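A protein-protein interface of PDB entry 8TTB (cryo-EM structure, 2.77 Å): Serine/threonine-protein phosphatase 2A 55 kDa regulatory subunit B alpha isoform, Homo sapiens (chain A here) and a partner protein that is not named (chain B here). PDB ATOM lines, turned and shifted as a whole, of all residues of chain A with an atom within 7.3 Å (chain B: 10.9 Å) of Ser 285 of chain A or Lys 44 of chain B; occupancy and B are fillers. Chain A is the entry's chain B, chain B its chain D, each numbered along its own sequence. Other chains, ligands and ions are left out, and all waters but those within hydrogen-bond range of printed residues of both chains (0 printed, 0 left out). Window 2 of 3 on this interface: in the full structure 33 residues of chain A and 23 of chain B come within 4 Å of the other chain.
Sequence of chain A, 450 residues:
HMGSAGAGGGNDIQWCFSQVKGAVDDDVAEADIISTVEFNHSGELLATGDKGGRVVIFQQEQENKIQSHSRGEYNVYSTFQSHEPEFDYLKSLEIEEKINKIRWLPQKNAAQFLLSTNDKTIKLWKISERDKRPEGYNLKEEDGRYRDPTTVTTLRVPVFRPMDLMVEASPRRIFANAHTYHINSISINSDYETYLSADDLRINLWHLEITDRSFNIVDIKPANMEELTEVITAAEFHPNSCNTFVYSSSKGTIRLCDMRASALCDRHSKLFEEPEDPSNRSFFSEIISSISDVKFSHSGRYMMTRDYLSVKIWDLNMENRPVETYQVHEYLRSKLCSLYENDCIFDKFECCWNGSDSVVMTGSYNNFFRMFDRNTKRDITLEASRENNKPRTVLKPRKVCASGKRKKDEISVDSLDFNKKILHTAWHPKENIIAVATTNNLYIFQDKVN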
ATOM      1  N   SER A 250     -32.887  25.340  15.347  1.00  0.00           N
ATOM      2  CA  SER A 250     -32.641  24.193  14.485  1.00  0.00           C
ATOM      3  C   SER A 250     -32.514  22.889  15.260  1.00  0.00           C
ATOM      4  O   SER A 250     -32.523  21.821  14.640  1.00  0.00           O
ATOM      5  CB  SER A 250     -31.377  24.423  13.660  1.00  0.00           C
ATOM      6  OG  SER A 250     -30.263  24.662  14.499  1.00  0.00           O
ATOM      7  N   LYS A 251     -32.394  22.946  16.585  1.00  0.00           N
ATOM      8  CA  LYS A 251     -32.351  21.739  17.400  1.00  0.00           C
ATOM      9  C   LYS A 251     -33.734  21.192  17.721  1.00  0.00           C
ATOM     10  O   LYS A 251     -33.830  20.125  18.334  1.00  0.00           O
ATOM     11  CB  LYS A 251     -31.601  22.010  18.706  1.00  0.00           C
ATOM     12  CG  LYS A 251     -30.095  22.118  18.551  1.00  0.00           C
ATOM     13  CD  LYS A 251     -29.434  22.489  19.868  1.00  0.00           C
ATOM     14  CE  LYS A 251     -27.924  22.591  19.735  1.00  0.00           C
ATOM     15  NZ  LYS A 251     -27.321  23.334  20.876  1.00  0.00           N
ATOM     16  N   ARG A 281     -34.049   7.757  16.476  1.00  0.00           N
ATOM     17  CA  ARG A 281     -32.621   8.047  16.434  1.00  0.00           C
ATOM     18  C   ARG A 281     -32.080   7.850  15.023  1.00  0.00           C
ATOM     19  O   ARG A 281     -31.115   7.115  14.812  1.00  0.00           O
ATOM     20  CB  ARG A 281     -31.864   7.157  17.421  1.00  0.00           C
ATOM     21  CG  ARG A 281     -32.366   7.263  18.850  1.00  0.00           C
ATOM     22  CD  ARG A 281     -31.577   6.367  19.789  1.00  0.00           C
ATOM     23  NE  ARG A 281     -32.081   6.440  21.156  1.00  0.00           N
ATOM     24  CZ  ARG A 281     -31.732   7.367  22.039  1.00  0.00           C
ATOM     25  NH1 ARG A 281     -30.870   8.324  21.735  1.00  0.00           N
ATOM     26  NH2 ARG A 281     -32.265   7.334  23.257  1.00  0.00           N
ATOM     27  N   SER A 282     -32.709   8.517  14.061  1.00  0.00           N
ATOM     28  CA  SER A 282     -32.336   8.356  12.664  1.00  0.00           C
ATOM     29  C   SER A 282     -30.997   9.028  12.377  1.00  0.00           C
ATOM     30  O   SER A 282     -30.496   9.846  13.153  1.00  0.00           O
ATOM     31  CB  SER A 282     -33.416   8.940  11.753  1.00  0.00           C
ATOM     32  OG  SER A 282     -33.052   8.813  10.390  1.00  0.00           O
ATOM     33  N   PHE A 283     -30.412   8.659  11.237  1.00  0.00           N
ATOM     34  CA  PHE A 283     -29.150   9.259  10.819  1.00  0.00           C
ATOM     35  C   PHE A 283     -29.310  10.755  10.575  1.00  0.00           C
ATOM     36  O   PHE A 283     -28.445  11.554  10.953  1.00  0.00           O
ATOM     37  CB  PHE A 283     -28.636   8.550   9.564  1.00  0.00           C
ATOM     38  CG  PHE A 283     -27.342   9.101   9.040  1.00  0.00           C
ATOM     39  CD1 PHE A 283     -26.154   8.870   9.711  1.00  0.00           C
ATOM     40  CD2 PHE A 283     -27.312   9.837   7.869  1.00  0.00           C
ATOM     41  CE1 PHE A 283     -24.962   9.372   9.228  1.00  0.00           C
ATOM     42  CE2 PHE A 283     -26.122  10.340   7.381  1.00  0.00           C
ATOM     43  CZ  PHE A 283     -24.946  10.108   8.061  1.00  0.00           C
ATOM     44  N   PHE A 284     -30.412  11.154   9.942  1.00  0.00           N
ATOM     45  CA  PHE A 284     -30.677  12.555   9.634  1.00  0.00           C
ATOM     46  C   PHE A 284     -31.411  13.284  10.751  1.00  0.00           C
ATOM     47  O   PHE A 284     -32.037  14.315  10.484  1.00  0.00           O
ATOM     48  CB  PHE A 284     -31.492  12.661   8.343  1.00  0.00           C
ATOM     49  CG  PHE A 284     -30.877  11.945   7.179  1.00  0.00           C
ATOM     50  CD1 PHE A 284     -29.972  12.587   6.355  1.00  0.00           C
ATOM     51  CD2 PHE A 284     -31.207  10.629   6.909  1.00  0.00           C
ATOM     52  CE1 PHE A 284     -29.406  11.931   5.283  1.00  0.00           C
ATOM     53  CE2 PHE A 284     -30.645   9.968   5.839  1.00  0.00           C
ATOM     54  CZ  PHE A 284     -29.744  10.619   5.025  1.00  0.00           C
ATOM     55  N   SER A 285     -31.351  12.781  11.985  1.00  0.00           N
ATOM     56  CA  SER A 285     -32.109  13.392  13.073  1.00  0.00           C
ATOM     57  C   SER A 285     -31.780  14.871  13.227  1.00  0.00           C
ATOM     58  O   SER A 285     -32.660  15.681  13.539  1.00  0.00           O
ATOM     59  CB  SER A 285     -31.835  12.647  14.380  1.00  0.00           C
ATOM     60  OG  SER A 285     -30.457  12.679  14.701  1.00  0.00           O
ATOM     61  N   GLU A 286     -30.517  15.244  13.019  1.00  0.00           N
ATOM     62  CA  GLU A 286     -30.125  16.637  13.205  1.00  0.00           C
ATOM     63  C   GLU A 286     -30.837  17.562  12.228  1.00  0.00           C
ATOM     64  O   GLU A 286     -30.991  18.756  12.507  1.00  0.00           O
ATOM     65  CB  GLU A 286     -28.610  16.779  13.054  1.00  0.00           C
ATOM     66  CG  GLU A 286     -27.809  15.902  14.001  1.00  0.00           C
ATOM     67  CD  GLU A 286     -28.086  16.210  15.459  1.00  0.00           C
ATOM     68  OE1 GLU A 286     -28.620  17.301  15.747  1.00  0.00           O
ATOM     69  OE2 GLU A 286     -27.772  15.359  16.318  1.00  0.00           O
ATOM     70  N   ILE A 287     -31.275  17.040  11.083  1.00  0.00           N
ATOM     71  CA  ILE A 287     -31.901  17.862  10.055  1.00  0.00           C
ATOM     72  C   ILE A 287     -33.411  17.874  10.252  1.00  0.00           C
ATOM     73  O   ILE A 287     -34.021  18.939  10.384  1.00  0.00           O
ATOM     74  CB  ILE A 287     -31.536  17.359   8.647  1.00  0.00           C
ATOM     75  CG1 ILE A 287     -30.021  17.425   8.441  1.00  0.00           C
ATOM     76  CG2 ILE A 287     -32.256  18.181   7.586  1.00  0.00           C
ATOM     77  CD1 ILE A 287     -29.548  16.815   7.139  1.00  0.00           C
ATOM     78  N   ILE A 288     -34.023  16.688  10.271  1.00  0.00           N
ATOM     79  CA  ILE A 288     -35.479  16.605  10.339  1.00  0.00           C
ATOM     80  C   ILE A 288     -36.002  17.191  11.643  1.00  0.00           C
ATOM     81  O   ILE A 288     -37.178  17.561  11.735  1.00  0.00           O
ATOM     82  CB  ILE A 288     -35.938  15.147  10.151  1.00  0.00           C
ATOM     83  CG1 ILE A 288     -35.389  14.259  11.271  1.00  0.00           C
ATOM     84  CG2 ILE A 288     -35.486  14.628   8.798  1.00  0.00           C
ATOM     85  CD1 ILE A 288     -35.858  12.824  11.191  1.00  0.00           C
ATOM     86  N   SER A 289     -35.156  17.275  12.672  1.00  0.00           N
ATOM     87  CA  SER A 289     -35.606  17.819  13.949  1.00  0.00           C
ATOM     88  C   SER A 289     -35.823  19.324  13.879  1.00  0.00           C
ATOM     89  O   SER A 289     -36.614  19.868  14.659  1.00  0.00           O
ATOM     90  CB  SER A 289     -34.596  17.483  15.045  1.00  0.00           C
ATOM     91  OG  SER A 289     -33.343  18.088  14.782  1.00  0.00           O
ATOM     92  N   SER A 290     -35.140  20.012  12.967  1.00  0.00           N
ATOM     93  CA  SER A 290     -35.255  21.461  12.870  1.00  0.00           C
ATOM     94  C   SER A 290     -36.702  21.877  12.641  1.00  0.00           C
ATOM     95  O   SER A 290     -37.423  21.260  11.851  1.00  0.00           O
ATOM     96  CB  SER A 290     -34.374  21.979  11.734  1.00  0.00           C
ATOM     97  OG  SER A 290     -34.467  23.387  11.620  1.00  0.00           O
ATOM     98  N   LEU A 336     -35.458   9.266   3.304  1.00  0.00           N
ATOM     99  CA  LEU A 336     -34.662  10.434   3.667  1.00  0.00           C
ATOM    100  C   LEU A 336     -33.332  10.454   2.924  1.00  0.00           C
ATOM    101  O   LEU A 336     -32.803  11.527   2.611  1.00  0.00           O
ATOM    102  CB  LEU A 336     -34.431  10.460   5.178  1.00  0.00           C
ATOM    103  CG  LEU A 336     -35.679  10.644   6.044  1.00  0.00           C
ATOM    104  CD1 LEU A 336     -35.326  10.537   7.515  1.00  0.00           C
ATOM    105  CD2 LEU A 336     -36.347  11.978   5.753  1.00  0.00           C
ATOM    106  N   ILE A 345     -34.716  17.563   1.532  1.00  0.00           N
ATOM    107  CA  ILE A 345     -34.824  17.389   2.974  1.00  0.00           C
ATOM    108  C   ILE A 345     -34.709  18.715   3.711  1.00  0.00           C
ATOM    109  O   ILE A 345     -35.076  18.801   4.887  1.00  0.00           O
ATOM    110  CB  ILE A 345     -33.759  16.388   3.466  1.00  0.00           C
ATOM    111  CG1 ILE A 345     -34.064  15.948   4.898  1.00  0.00           C
ATOM    112  CG2 ILE A 345     -32.372  17.002   3.388  1.00  0.00           C
ATOM    113  CD1 ILE A 345     -33.185  14.821   5.389  1.00  0.00           C
ATOM    114  N   LYS B  44     -23.231  12.063  12.057  1.00  0.00           N
ATOM    115  CA  LYS B  44     -24.485  12.558  11.502  1.00  0.00           C
ATOM    116  C   LYS B  44     -24.219  13.658  10.475  1.00  0.00           C
ATOM    117  O   LYS B  44     -23.180  14.315  10.521  1.00  0.00           O
ATOM    118  CB  LYS B  44     -25.392  13.078  12.618  1.00  0.00           C
ATOM    119  CG  LYS B  44     -25.797  12.013  13.625  1.00  0.00           C
ATOM    120  CD  LYS B  44     -26.796  12.551  14.633  1.00  0.00           C
ATOM    121  CE  LYS B  44     -27.115  11.524  15.704  1.00  0.00           C
ATOM    122  NZ  LYS B  44     -28.084  12.045  16.707  1.00  0.00           N
ATOM    123  N   PRO B  45     -25.159  13.859   9.545  1.00  0.00           N
ATOM    124  CA  PRO B  45     -24.938  14.834   8.468  1.00  0.00           C
ATOM    125  C   PRO B  45     -25.094  16.284   8.896  1.00  0.00           C
ATOM    126  O   PRO B  45     -24.904  17.176   8.062  1.00  0.00           O
ATOM    127  CB  PRO B  45     -26.002  14.448   7.434  1.00  0.00           C
ATOM    128  CG  PRO B  45     -27.108  13.878   8.243  1.00  0.00           C
ATOM    129  CD  PRO B  45     -26.479  13.211   9.437  1.00  0.00           C
ATOM    130  N   GLY B  46     -25.441  16.551  10.153  1.00  0.00           N
ATOM    131  CA  GLY B  46     -25.557  17.916  10.627  1.00  0.00           C
ATOM    132  C   GLY B  46     -24.233  18.481  11.097  1.00  0.00           C
ATOM    133  O   GLY B  46     -23.235  18.424  10.374  1.00  0.00           O
ATOM    134  N   GLY B  47     -24.212  19.034  12.309  1.00  0.00           N
ATOM    135  CA  GLY B  47     -22.993  19.560  12.884  1.00  0.00           C
ATOM    136  C   GLY B  47     -22.860  21.060  12.728  1.00  0.00           C
ATOM    137  O   GLY B  47     -23.681  21.745  12.112  1.00  0.00           O
ATOM    138  N   SER B  48     -21.780  21.579  13.317  1.00  0.00           N
ATOM    139  CA  SER B  48     -21.537  23.017  13.291  1.00  0.00           C
ATOM    140  C   SER B  48     -21.252  23.502  11.875  1.00  0.00           C
ATOM    141  O   SER B  48     -21.857  24.471  11.403  1.00  0.00           O
ATOM    142  CB  SER B  48     -20.375  23.366  14.221  1.00  0.00           C
ATOM    143  OG  SER B  48     -20.114  24.757  14.209  1.00  0.00           O
ATOM    144  N   ASP B  49     -20.328  22.837  11.178  1.00  0.00           N
ATOM    145  CA  ASP B  49     -19.970  23.271   9.833  1.00  0.00           C
ATOM    146  C   ASP B  49     -21.161  23.197   8.890  1.00  0.00           C
ATOM    147  O   ASP B  49     -21.253  23.986   7.943  1.00  0.00           O
ATOM    148  CB  ASP B  49     -18.816  22.424   9.297  1.00  0.00           C
ATOM    149  CG  ASP B  49     -17.493  22.756   9.962  1.00  0.00           C
ATOM    150  OD1 ASP B  49     -17.466  23.665  10.817  1.00  0.00           O
ATOM    151  OD2 ASP B  49     -16.479  22.108   9.628  1.00  0.00           O
ATOM    152  N   PHE B  50     -22.078  22.259   9.126  1.00  0.00           N
ATOM    153  CA  PHE B  50     -23.275  22.176   8.298  1.00  0.00           C
ATOM    154  C   PHE B  50     -24.095  23.456   8.394  1.00  0.00           C
ATOM    155  O   PHE B  50     -24.547  23.995   7.378  1.00  0.00           O
ATOM    156  CB  PHE B  50     -24.105  20.966   8.715  1.00  0.00           C
ATOM    157  CG  PHE B  50     -25.559  21.096   8.395  1.00  0.00           C
ATOM    158  CD1 PHE B  50     -25.997  21.042   7.087  1.00  0.00           C
ATOM    159  CD2 PHE B  50     -26.487  21.271   9.405  1.00  0.00           C
ATOM    160  CE1 PHE B  50     -27.335  21.163   6.790  1.00  0.00           C
ATOM    161  CE2 PHE B  50     -27.828  21.391   9.114  1.00  0.00           C
ATOM    162  CZ  PHE B  50     -28.254  21.338   7.804  1.00  0.00           C
ATOM    163  N   LEU B  51     -24.300  23.958   9.612  1.00  0.00           N
ATOM    164  CA  LEU B  51     -25.049  25.198   9.783  1.00  0.00           C
ATOM    165  C   LEU B  51     -24.295  26.382   9.192  1.00  0.00           C
ATOM    166  O   LEU B  51     -24.884  27.229   8.511  1.00  0.00           O
ATOM    167  CB  LEU B  51     -25.340  25.434  11.264  1.00  0.00           C
ATOM    168  CG  LEU B  51     -26.186  24.364  11.953  1.00  0.00           C
ATOM    169  CD1 LEU B  51     -26.297  24.653  13.439  1.00  0.00           C
ATOM    170  CD2 LEU B  51     -27.565  24.275  11.321  1.00  0.00           C
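Of the 14 printed residues of chain A, 5 touch a printed residue of chain B.
Printed residues of chain A that touch a printed residue of chain B: Phe 283, Phe 284, Ser 285, Glu 286 and Ile 287.
Along chain A the printed residues that touch a printed residue of chain B span positions 283 to 287.
Of the 8 printed residues of chain B, 2 touch a printed residue of chain A.
Among the printed residues, Asp or Glu carboxylates within 4 Å of a Lys or Arg side-chain nitrogen of the other chain: Glu 286 of chain A with Lys 44 of chain B (3.4 Å).
Among the printed residues, merely in contact across the chains: Phe 283 of chain A with Lys 44 of chain B (3.8 Å), Phe 283 of chain A with Pro 45 of chain B (3.0 Å), Phe 284 of chain A with Pro 45 of chain B (3.7 Å) and Ile 287 of chain A with Pro 45 of chain B (3.97 Å).
Of the printed residues of chain B, Phe 284 of chain A touches Pro 45 (3.7 Å).
Of chain B, only Lys 44 comes within 4 Å of Glu 286 of chain A.
Ile 287 of chain A touches one residue of chain B.
No residue of chain B comes within 4 Å of Ser 289 of chain A.
Lys 44 of chain B touches three residues of chain A.
Of the printed residues of chain A, Pro 45 of chain B touches Phe 283 (3.0 Å), Phe 284 (3.7 Å) and Ile 287 (3.97 Å).
Gly 46 of chain B touches none of the printed residues of chain A.
Gly 47 of chain B touches none of the printed residues of chain A.
The side-chain amino group (NZ) of Lys 44 of chain B sits at hydrogen-bond distance from the side-chain hydroxyl (OG) of Ser 285 of chain A (3.2 Å).
OE2 of Glu 286 of chain A is in salt-bridge range of NZ of Lys 44 of chain B (3.4 Å).
O of Ser 282 of chain A is in hydrogen-bond range of OG of Ser 285 of chain A.
The backbone carbonyl oxygen (O) of Ser 285 of chain A lies within hydrogen-bond range of the side-chain hydroxyl (OG) of Ser 289 of chain A (2.8 Å).
The backbone carbonyl oxygen of Glu 286 of chain A is in hydrogen-bond range of the side-chain hydroxyl of Ser 289 of chain A (3.3 Å).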
